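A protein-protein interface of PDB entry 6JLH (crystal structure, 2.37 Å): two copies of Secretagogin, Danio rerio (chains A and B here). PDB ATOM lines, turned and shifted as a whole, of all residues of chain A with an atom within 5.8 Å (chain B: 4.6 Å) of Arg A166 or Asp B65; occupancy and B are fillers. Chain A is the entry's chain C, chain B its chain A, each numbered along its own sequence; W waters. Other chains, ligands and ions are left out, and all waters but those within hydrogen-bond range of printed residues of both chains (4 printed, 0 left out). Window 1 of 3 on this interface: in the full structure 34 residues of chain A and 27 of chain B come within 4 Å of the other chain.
The guanidinium group of Arg A166 is in hydrogen-bond range of the backbone carbonyl oxygen of Leu A170 (3.0 Å).
The side-chain carboxylate of Glu A172 is in salt-bridge range of the guanidinium group of Arg A166, 3.3 Å away.
Among the printed residues, merely in contact across the chains: Arg A166 with Asp B65 (3.9 Å) and Arg A166 with Arg B67 (3.6 Å).
Leu A161 touches none of the printed residues of chain B.
Of chain B, only Asp B65 (3.9 Å) and Arg B67 (3.6 Å) come within 4 Å of Arg A166.
Of chain A, only Arg A166 (3.9 Å) comes within 4 Å of Asp B65.
Of the printed residues of chain A, Arg B67 touches Arg A166.
The nearest printed residue of chain A that does not touch Asp B65 is Ala A169 (6.0 Å).
Of the 13 printed residues of chain A, 1 touches a printed residue of chain B.
Among the printed residues, 2 pairs touch across the chains.
No position is printed for both chains.
Of the 2 pairs that touch across the chains among the printed residues, none has its exchanged pair printed and touching as well.
Water W4 lies within hydrogen-bond range of O of Asp B65 (2.5 Å) and NH1 of Arg A166 (2.8 Å).
Water W3 lies within hydrogen-bond range of N of Glu A172 (2.6 Å) and NH1 of Arg B67 (3.4 Å).
Water W1 bridges NH1 of Arg B67 and OE1 of Glu A172.
Water W2 lies within hydrogen-bond range of OE1 of Glu A172 and NH2 of Arg B67.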
ATOM      1  N   PHE A 151       0.993 -24.444 -24.614  1.00  0.00           N
ATOM      2  CA  PHE A 151       0.333 -25.061 -25.796  1.00  0.00           C
ATOM      3  C   PHE A 151       1.341 -25.916 -26.584  1.00  0.00           C
ATOM      4  O   PHE A 151       0.906 -26.649 -27.455  1.00  0.00           O
ATOM      5  CB  PHE A 151      -0.338 -23.997 -26.675  1.00  0.00           C
ATOM      6  CG  PHE A 151      -1.625 -23.440 -26.104  1.00  0.00           C
ATOM      7  CD1 PHE A 151      -2.779 -24.204 -26.124  1.00  0.00           C
ATOM      8  CD2 PHE A 151      -1.685 -22.157 -25.540  1.00  0.00           C
ATOM      9  CE1 PHE A 151      -3.960 -23.716 -25.572  1.00  0.00           C
ATOM     10  CE2 PHE A 151      -2.862 -21.688 -24.972  1.00  0.00           C
ATOM     11  CZ  PHE A 151      -3.999 -22.460 -24.998  1.00  0.00           C
ATOM     12  N   LEU A 161       0.077 -27.441 -36.136  1.00  0.00           N
ATOM     13  CA  LEU A 161      -1.227 -27.069 -36.713  1.00  0.00           C
ATOM     14  C   LEU A 161      -2.349 -27.299 -35.685  1.00  0.00           C
ATOM     15  O   LEU A 161      -3.165 -26.389 -35.526  1.00  0.00           O
ATOM     16  CB  LEU A 161      -1.377 -27.928 -37.968  1.00  0.00           C
ATOM     17  CG  LEU A 161      -2.582 -27.620 -38.837  1.00  0.00           C
ATOM     18  CD1 LEU A 161      -2.373 -26.266 -39.497  1.00  0.00           C
ATOM     19  CD2 LEU A 161      -2.760 -28.727 -39.866  1.00  0.00           C
ATOM     20  N   ASN A 162      -2.399 -28.463 -35.032  1.00  0.00           N
ATOM     21  CA  ASN A 162      -3.468 -28.840 -34.077  1.00  0.00           C
ATOM     22  C   ASN A 162      -3.355 -28.001 -32.780  1.00  0.00           C
ATOM     23  O   ASN A 162      -4.404 -27.807 -32.079  1.00  0.00           O
ATOM     24  CB  ASN A 162      -3.456 -30.343 -33.799  1.00  0.00           C
ATOM     25  CG  ASN A 162      -2.151 -30.815 -33.182  1.00  0.00           C
ATOM     26  OD1 ASN A 162      -1.085 -30.552 -33.713  1.00  0.00           O
ATOM     27  ND2 ASN A 162      -2.198 -31.500 -32.058  1.00  0.00           N
ATOM     28  N   ASP A 163      -2.179 -27.463 -32.478  1.00  0.00           N
ATOM     29  CA  ASP A 163      -2.003 -26.574 -31.303  1.00  0.00           C
ATOM     30  C   ASP A 163      -2.721 -25.253 -31.597  1.00  0.00           C
ATOM     31  O   ASP A 163      -3.461 -24.752 -30.697  1.00  0.00           O
ATOM     32  CB  ASP A 163      -0.522 -26.376 -30.962  1.00  0.00           C
ATOM     33  CG  ASP A 163       0.211 -27.681 -30.662  1.00  0.00           C
ATOM     34  OD1 ASP A 163      -0.398 -28.578 -30.059  1.00  0.00           O
ATOM     35  OD2 ASP A 163       1.394 -27.779 -31.007  1.00  0.00           O
ATOM     36  N   LEU A 164      -2.530 -24.703 -32.800  1.00  0.00           N
ATOM     37  CA  LEU A 164      -3.154 -23.408 -33.169  1.00  0.00           C
ATOM     38  C   LEU A 164      -4.671 -23.598 -33.272  1.00  0.00           C
ATOM     39  O   LEU A 164      -5.397 -22.730 -32.783  1.00  0.00           O
ATOM     40  CB  LEU A 164      -2.591 -22.870 -34.485  1.00  0.00           C
ATOM     41  CG  LEU A 164      -3.042 -21.443 -34.774  1.00  0.00           C
ATOM     42  CD1 LEU A 164      -2.470 -20.474 -33.763  1.00  0.00           C
ATOM     43  CD2 LEU A 164      -2.662 -21.007 -36.169  1.00  0.00           C
ATOM     44  N   ALA A 165      -5.123 -24.707 -33.866  1.00  0.00           N
ATOM     45  CA  ALA A 165      -6.536 -25.120 -33.890  1.00  0.00           C
ATOM     46  C   ALA A 165      -7.137 -25.015 -32.487  1.00  0.00           C
ATOM     47  O   ALA A 165      -8.236 -24.479 -32.398  1.00  0.00           O
ATOM     48  CB  ALA A 165      -6.670 -26.524 -34.409  1.00  0.00           C
ATOM     49  N   ARG A 166      -6.471 -25.576 -31.464  1.00  0.00           N
ATOM     50  CA  ARG A 166      -6.991 -25.612 -30.074  1.00  0.00           C
ATOM     51  C   ARG A 166      -6.995 -24.171 -29.536  1.00  0.00           C
ATOM     52  O   ARG A 166      -8.015 -23.768 -28.986  1.00  0.00           O
ATOM     53  CB  ARG A 166      -6.212 -26.571 -29.160  1.00  0.00           C
ATOM     54  CG  ARG A 166      -6.554 -28.044 -29.310  1.00  0.00           C
ATOM     55  CD  ARG A 166      -8.057 -28.350 -29.368  1.00  0.00           C
ATOM     56  NE  ARG A 166      -8.537 -28.504 -30.738  1.00  0.00           N
ATOM     57  CZ  ARG A 166      -9.675 -27.991 -31.213  1.00  0.00           C
ATOM     58  NH1 ARG A 166     -10.468 -27.224 -30.461  1.00  0.00           N
ATOM     59  NH2 ARG A 166     -10.015 -28.248 -32.468  1.00  0.00           N
ATOM     60  N   ILE A 167      -5.941 -23.400 -29.776  1.00  0.00           N
ATOM     61  CA  ILE A 167      -5.858 -21.978 -29.335  1.00  0.00           C
ATOM     62  C   ILE A 167      -7.034 -21.162 -29.895  1.00  0.00           C
ATOM     63  O   ILE A 167      -7.576 -20.348 -29.146  1.00  0.00           O
ATOM     64  CB  ILE A 167      -4.500 -21.358 -29.700  1.00  0.00           C
ATOM     65  CG1 ILE A 167      -3.389 -21.948 -28.831  1.00  0.00           C
ATOM     66  CG2 ILE A 167      -4.578 -19.832 -29.590  1.00  0.00           C
ATOM     67  CD1 ILE A 167      -1.979 -21.600 -29.305  1.00  0.00           C
ATOM     68  N   LEU A 168      -7.437 -21.400 -31.146  1.00  0.00           N
ATOM     69  CA  LEU A 168      -8.466 -20.604 -31.885  1.00  0.00           C
ATOM     70  C   LEU A 168      -9.831 -21.281 -31.811  1.00  0.00           C
ATOM     71  O   LEU A 168     -10.747 -20.778 -32.408  1.00  0.00           O
ATOM     72  CB  LEU A 168      -8.012 -20.437 -33.333  1.00  0.00           C
ATOM     73  CG  LEU A 168      -6.686 -19.694 -33.496  1.00  0.00           C
ATOM     74  CD1 LEU A 168      -6.260 -19.602 -34.949  1.00  0.00           C
ATOM     75  CD2 LEU A 168      -6.771 -18.303 -32.905  1.00  0.00           C
ATOM     76  N   ALA A 169      -9.969 -22.370 -31.063  1.00  0.00           N
ATOM     77  CA  ALA A 169     -11.254 -23.071 -30.840  1.00  0.00           C
ATOM     78  C   ALA A 169     -11.856 -23.493 -32.184  1.00  0.00           C
ATOM     79  O   ALA A 169     -13.082 -23.364 -32.336  1.00  0.00           O
ATOM     80  CB  ALA A 169     -12.204 -22.183 -30.049  1.00  0.00           C
ATOM     81  N   LEU A 170     -11.038 -23.971 -33.119  1.00  0.00           N
ATOM     82  CA  LEU A 170     -11.531 -24.423 -34.449  1.00  0.00           C
ATOM     83  C   LEU A 170     -12.557 -25.534 -34.195  1.00  0.00           C
ATOM     84  O   LEU A 170     -12.264 -26.431 -33.416  1.00  0.00           O
ATOM     85  CB  LEU A 170     -10.356 -24.903 -35.326  1.00  0.00           C
ATOM     86  CG  LEU A 170     -10.749 -25.543 -36.662  1.00  0.00           C
ATOM     87  CD1 LEU A 170     -11.371 -24.495 -37.596  1.00  0.00           C
ATOM     88  CD2 LEU A 170      -9.551 -26.221 -37.323  1.00  0.00           C
ATOM     89  N   GLN A 171     -13.726 -25.434 -34.817  1.00  0.00           N
ATOM     90  CA  GLN A 171     -14.788 -26.464 -34.789  1.00  0.00           C
ATOM     91  C   GLN A 171     -14.636 -27.302 -36.054  1.00  0.00           C
ATOM     92  O   GLN A 171     -14.579 -26.687 -37.114  1.00  0.00           O
ATOM     93  CB  GLN A 171     -16.136 -25.765 -34.635  1.00  0.00           C
ATOM     94  CG  GLN A 171     -16.387 -25.360 -33.181  1.00  0.00           C
ATOM     95  CD  GLN A 171     -17.593 -24.482 -32.997  1.00  0.00           C
ATOM     96  OE1 GLN A 171     -18.402 -24.312 -33.905  1.00  0.00           O
ATOM     97  NE2 GLN A 171     -17.715 -23.910 -31.811  1.00  0.00           N
ATOM     98  N   GLU A 172     -14.468 -28.622 -35.942  1.00  0.00           N
ATOM     99  CA  GLU A 172     -14.070 -29.439 -37.126  1.00  0.00           C
ATOM    100  C   GLU A 172     -15.098 -30.501 -37.529  1.00  0.00           C
ATOM    101  O   GLU A 172     -14.666 -31.603 -37.909  1.00  0.00           O
ATOM    102  CB  GLU A 172     -12.724 -30.108 -36.839  1.00  0.00           C
ATOM    103  CG  GLU A 172     -11.736 -29.195 -36.132  1.00  0.00           C
ATOM    104  CD  GLU A 172     -10.530 -29.893 -35.528  1.00  0.00           C
ATOM    105  OE1 GLU A 172     -10.682 -31.034 -35.066  1.00  0.00           O
ATOM    106  OE2 GLU A 172      -9.441 -29.295 -35.526  1.00  0.00           O
ATOM    107  N   TYR B  21     -17.980 -33.628 -28.246  1.00  0.00           N
ATOM    108  CA  TYR B  21     -17.476 -32.457 -27.483  1.00  0.00           C
ATOM    109  C   TYR B  21     -18.620 -31.487 -27.189  1.00  0.00           C
ATOM    110  O   TYR B  21     -19.359 -31.157 -28.119  1.00  0.00           O
ATOM    111  CB  TYR B  21     -16.400 -31.702 -28.269  1.00  0.00           C
ATOM    112  CG  TYR B  21     -15.142 -32.491 -28.517  1.00  0.00           C
ATOM    113  CD1 TYR B  21     -14.232 -32.711 -27.501  1.00  0.00           C
ATOM    114  CD2 TYR B  21     -14.879 -33.055 -29.756  1.00  0.00           C
ATOM    115  CE1 TYR B  21     -13.085 -33.467 -27.703  1.00  0.00           C
ATOM    116  CE2 TYR B  21     -13.728 -33.799 -29.983  1.00  0.00           C
ATOM    117  CZ  TYR B  21     -12.818 -33.999 -28.956  1.00  0.00           C
ATOM    118  OH  TYR B  21     -11.688 -34.744 -29.158  1.00  0.00           O
ATOM    119  N   ASP B  61     -11.943 -29.579 -16.895  1.00  0.00           N
ATOM    120  CA  ASP B  61     -11.367 -29.657 -18.262  1.00  0.00           C
ATOM    121  C   ASP B  61      -9.963 -30.248 -18.151  1.00  0.00           C
ATOM    122  O   ASP B  61      -8.989 -29.510 -18.361  1.00  0.00           O
ATOM    123  CB  ASP B  61     -11.373 -28.311 -18.988  1.00  0.00           C
ATOM    124  CG  ASP B  61     -10.889 -28.429 -20.425  1.00  0.00           C
ATOM    125  OD1 ASP B  61     -10.696 -29.576 -20.882  1.00  0.00           O
ATOM    126  OD2 ASP B  61     -10.706 -27.380 -21.085  1.00  0.00           O
ATOM    127  N   THR B  63      -8.330 -32.170 -20.171  1.00  0.00           N
ATOM    128  CA  THR B  63      -7.548 -32.237 -21.442  1.00  0.00           C
ATOM    129  C   THR B  63      -7.090 -30.836 -21.873  1.00  0.00           C
ATOM    130  O   THR B  63      -6.300 -30.768 -22.838  1.00  0.00           O
ATOM    131  CB  THR B  63      -8.321 -32.943 -22.569  1.00  0.00           C
ATOM    132  OG1 THR B  63      -9.426 -32.138 -22.975  1.00  0.00           O
ATOM    133  CG2 THR B  63      -8.793 -34.331 -22.179  1.00  0.00           C
ATOM    134  N   PHE B  64      -7.575 -29.775 -21.220  1.00  0.00           N
ATOM    135  CA  PHE B  64      -7.120 -28.361 -21.365  1.00  0.00           C
ATOM    136  C   PHE B  64      -7.328 -27.827 -22.785  1.00  0.00           C
ATOM    137  O   PHE B  64      -6.478 -27.124 -23.266  1.00  0.00           O
ATOM    138  CB  PHE B  64      -5.652 -28.225 -20.960  1.00  0.00           C
ATOM    139  CG  PHE B  64      -5.405 -28.740 -19.571  1.00  0.00           C
ATOM    140  CD1 PHE B  64      -5.840 -28.008 -18.479  1.00  0.00           C
ATOM    141  CD2 PHE B  64      -4.776 -29.962 -19.362  1.00  0.00           C
ATOM    142  CE1 PHE B  64      -5.625 -28.482 -17.198  1.00  0.00           C
ATOM    143  CE2 PHE B  64      -4.587 -30.448 -18.082  1.00  0.00           C
ATOM    144  CZ  PHE B  64      -5.015 -29.707 -17.005  1.00  0.00           C
ATOM    145  N   ASP B  65      -8.487 -28.084 -23.388  1.00  0.00           N
ATOM    146  CA  ASP B  65      -8.811 -27.708 -24.791  1.00  0.00           C
ATOM    147  C   ASP B  65      -9.993 -26.734 -24.812  1.00  0.00           C
ATOM    148  O   ASP B  65     -10.381 -26.301 -25.915  1.00  0.00           O
ATOM    149  CB  ASP B  65      -9.074 -28.973 -25.627  1.00  0.00           C
ATOM    150  CG  ASP B  65     -10.253 -29.814 -25.149  1.00  0.00           C
ATOM    151  OD1 ASP B  65     -10.725 -29.610 -24.002  1.00  0.00           O
ATOM    152  OD2 ASP B  65     -10.690 -30.675 -25.928  1.00  0.00           O
ATOM    153  N   GLY B  66     -10.559 -26.397 -23.650  1.00  0.00           N
ATOM    154  CA  GLY B  66     -11.688 -25.441 -23.551  1.00  0.00           C
ATOM    155  C   GLY B  66     -13.013 -26.069 -23.963  1.00  0.00           C
ATOM    156  O   GLY B  66     -14.002 -25.340 -24.112  1.00  0.00           O
ATOM    157  N   ARG B  67     -13.039 -27.396 -24.102  1.00  0.00           N
ATOM    158  CA  ARG B  67     -14.242 -28.203 -24.423  1.00  0.00           C
ATOM    159  C   ARG B  67     -14.450 -29.267 -23.344  1.00  0.00           C
ATOM    160  O   ARG B  67     -13.465 -29.674 -22.714  1.00  0.00           O
ATOM    161  CB  ARG B  67     -14.065 -28.949 -25.748  1.00  0.00           C
ATOM    162  CG  ARG B  67     -13.382 -28.151 -26.844  1.00  0.00           C
ATOM    163  CD  ARG B  67     -13.451 -28.879 -28.174  1.00  0.00           C
ATOM    164  NE  ARG B  67     -12.332 -29.788 -28.347  1.00  0.00           N
ATOM    165  CZ  ARG B  67     -11.995 -30.344 -29.505  1.00  0.00           C
ATOM    166  NH1 ARG B  67     -12.699 -30.102 -30.601  1.00  0.00           N
ATOM    167  NH2 ARG B  67     -10.956 -31.154 -29.566  1.00  0.00           N
HETATM  168  O   HOH W   1     -12.676 -31.509 -33.075  1.00  0.00           O
HETATM  169  O   HOH W   2      -9.409 -31.695 -32.365  1.00  0.00           O
HETATM  170  O   HOH W   3     -14.472 -29.509 -33.451  1.00  0.00           O
HETATM  171  O   HOH W   4     -10.073 -25.556 -28.255  1.00  0.00           O
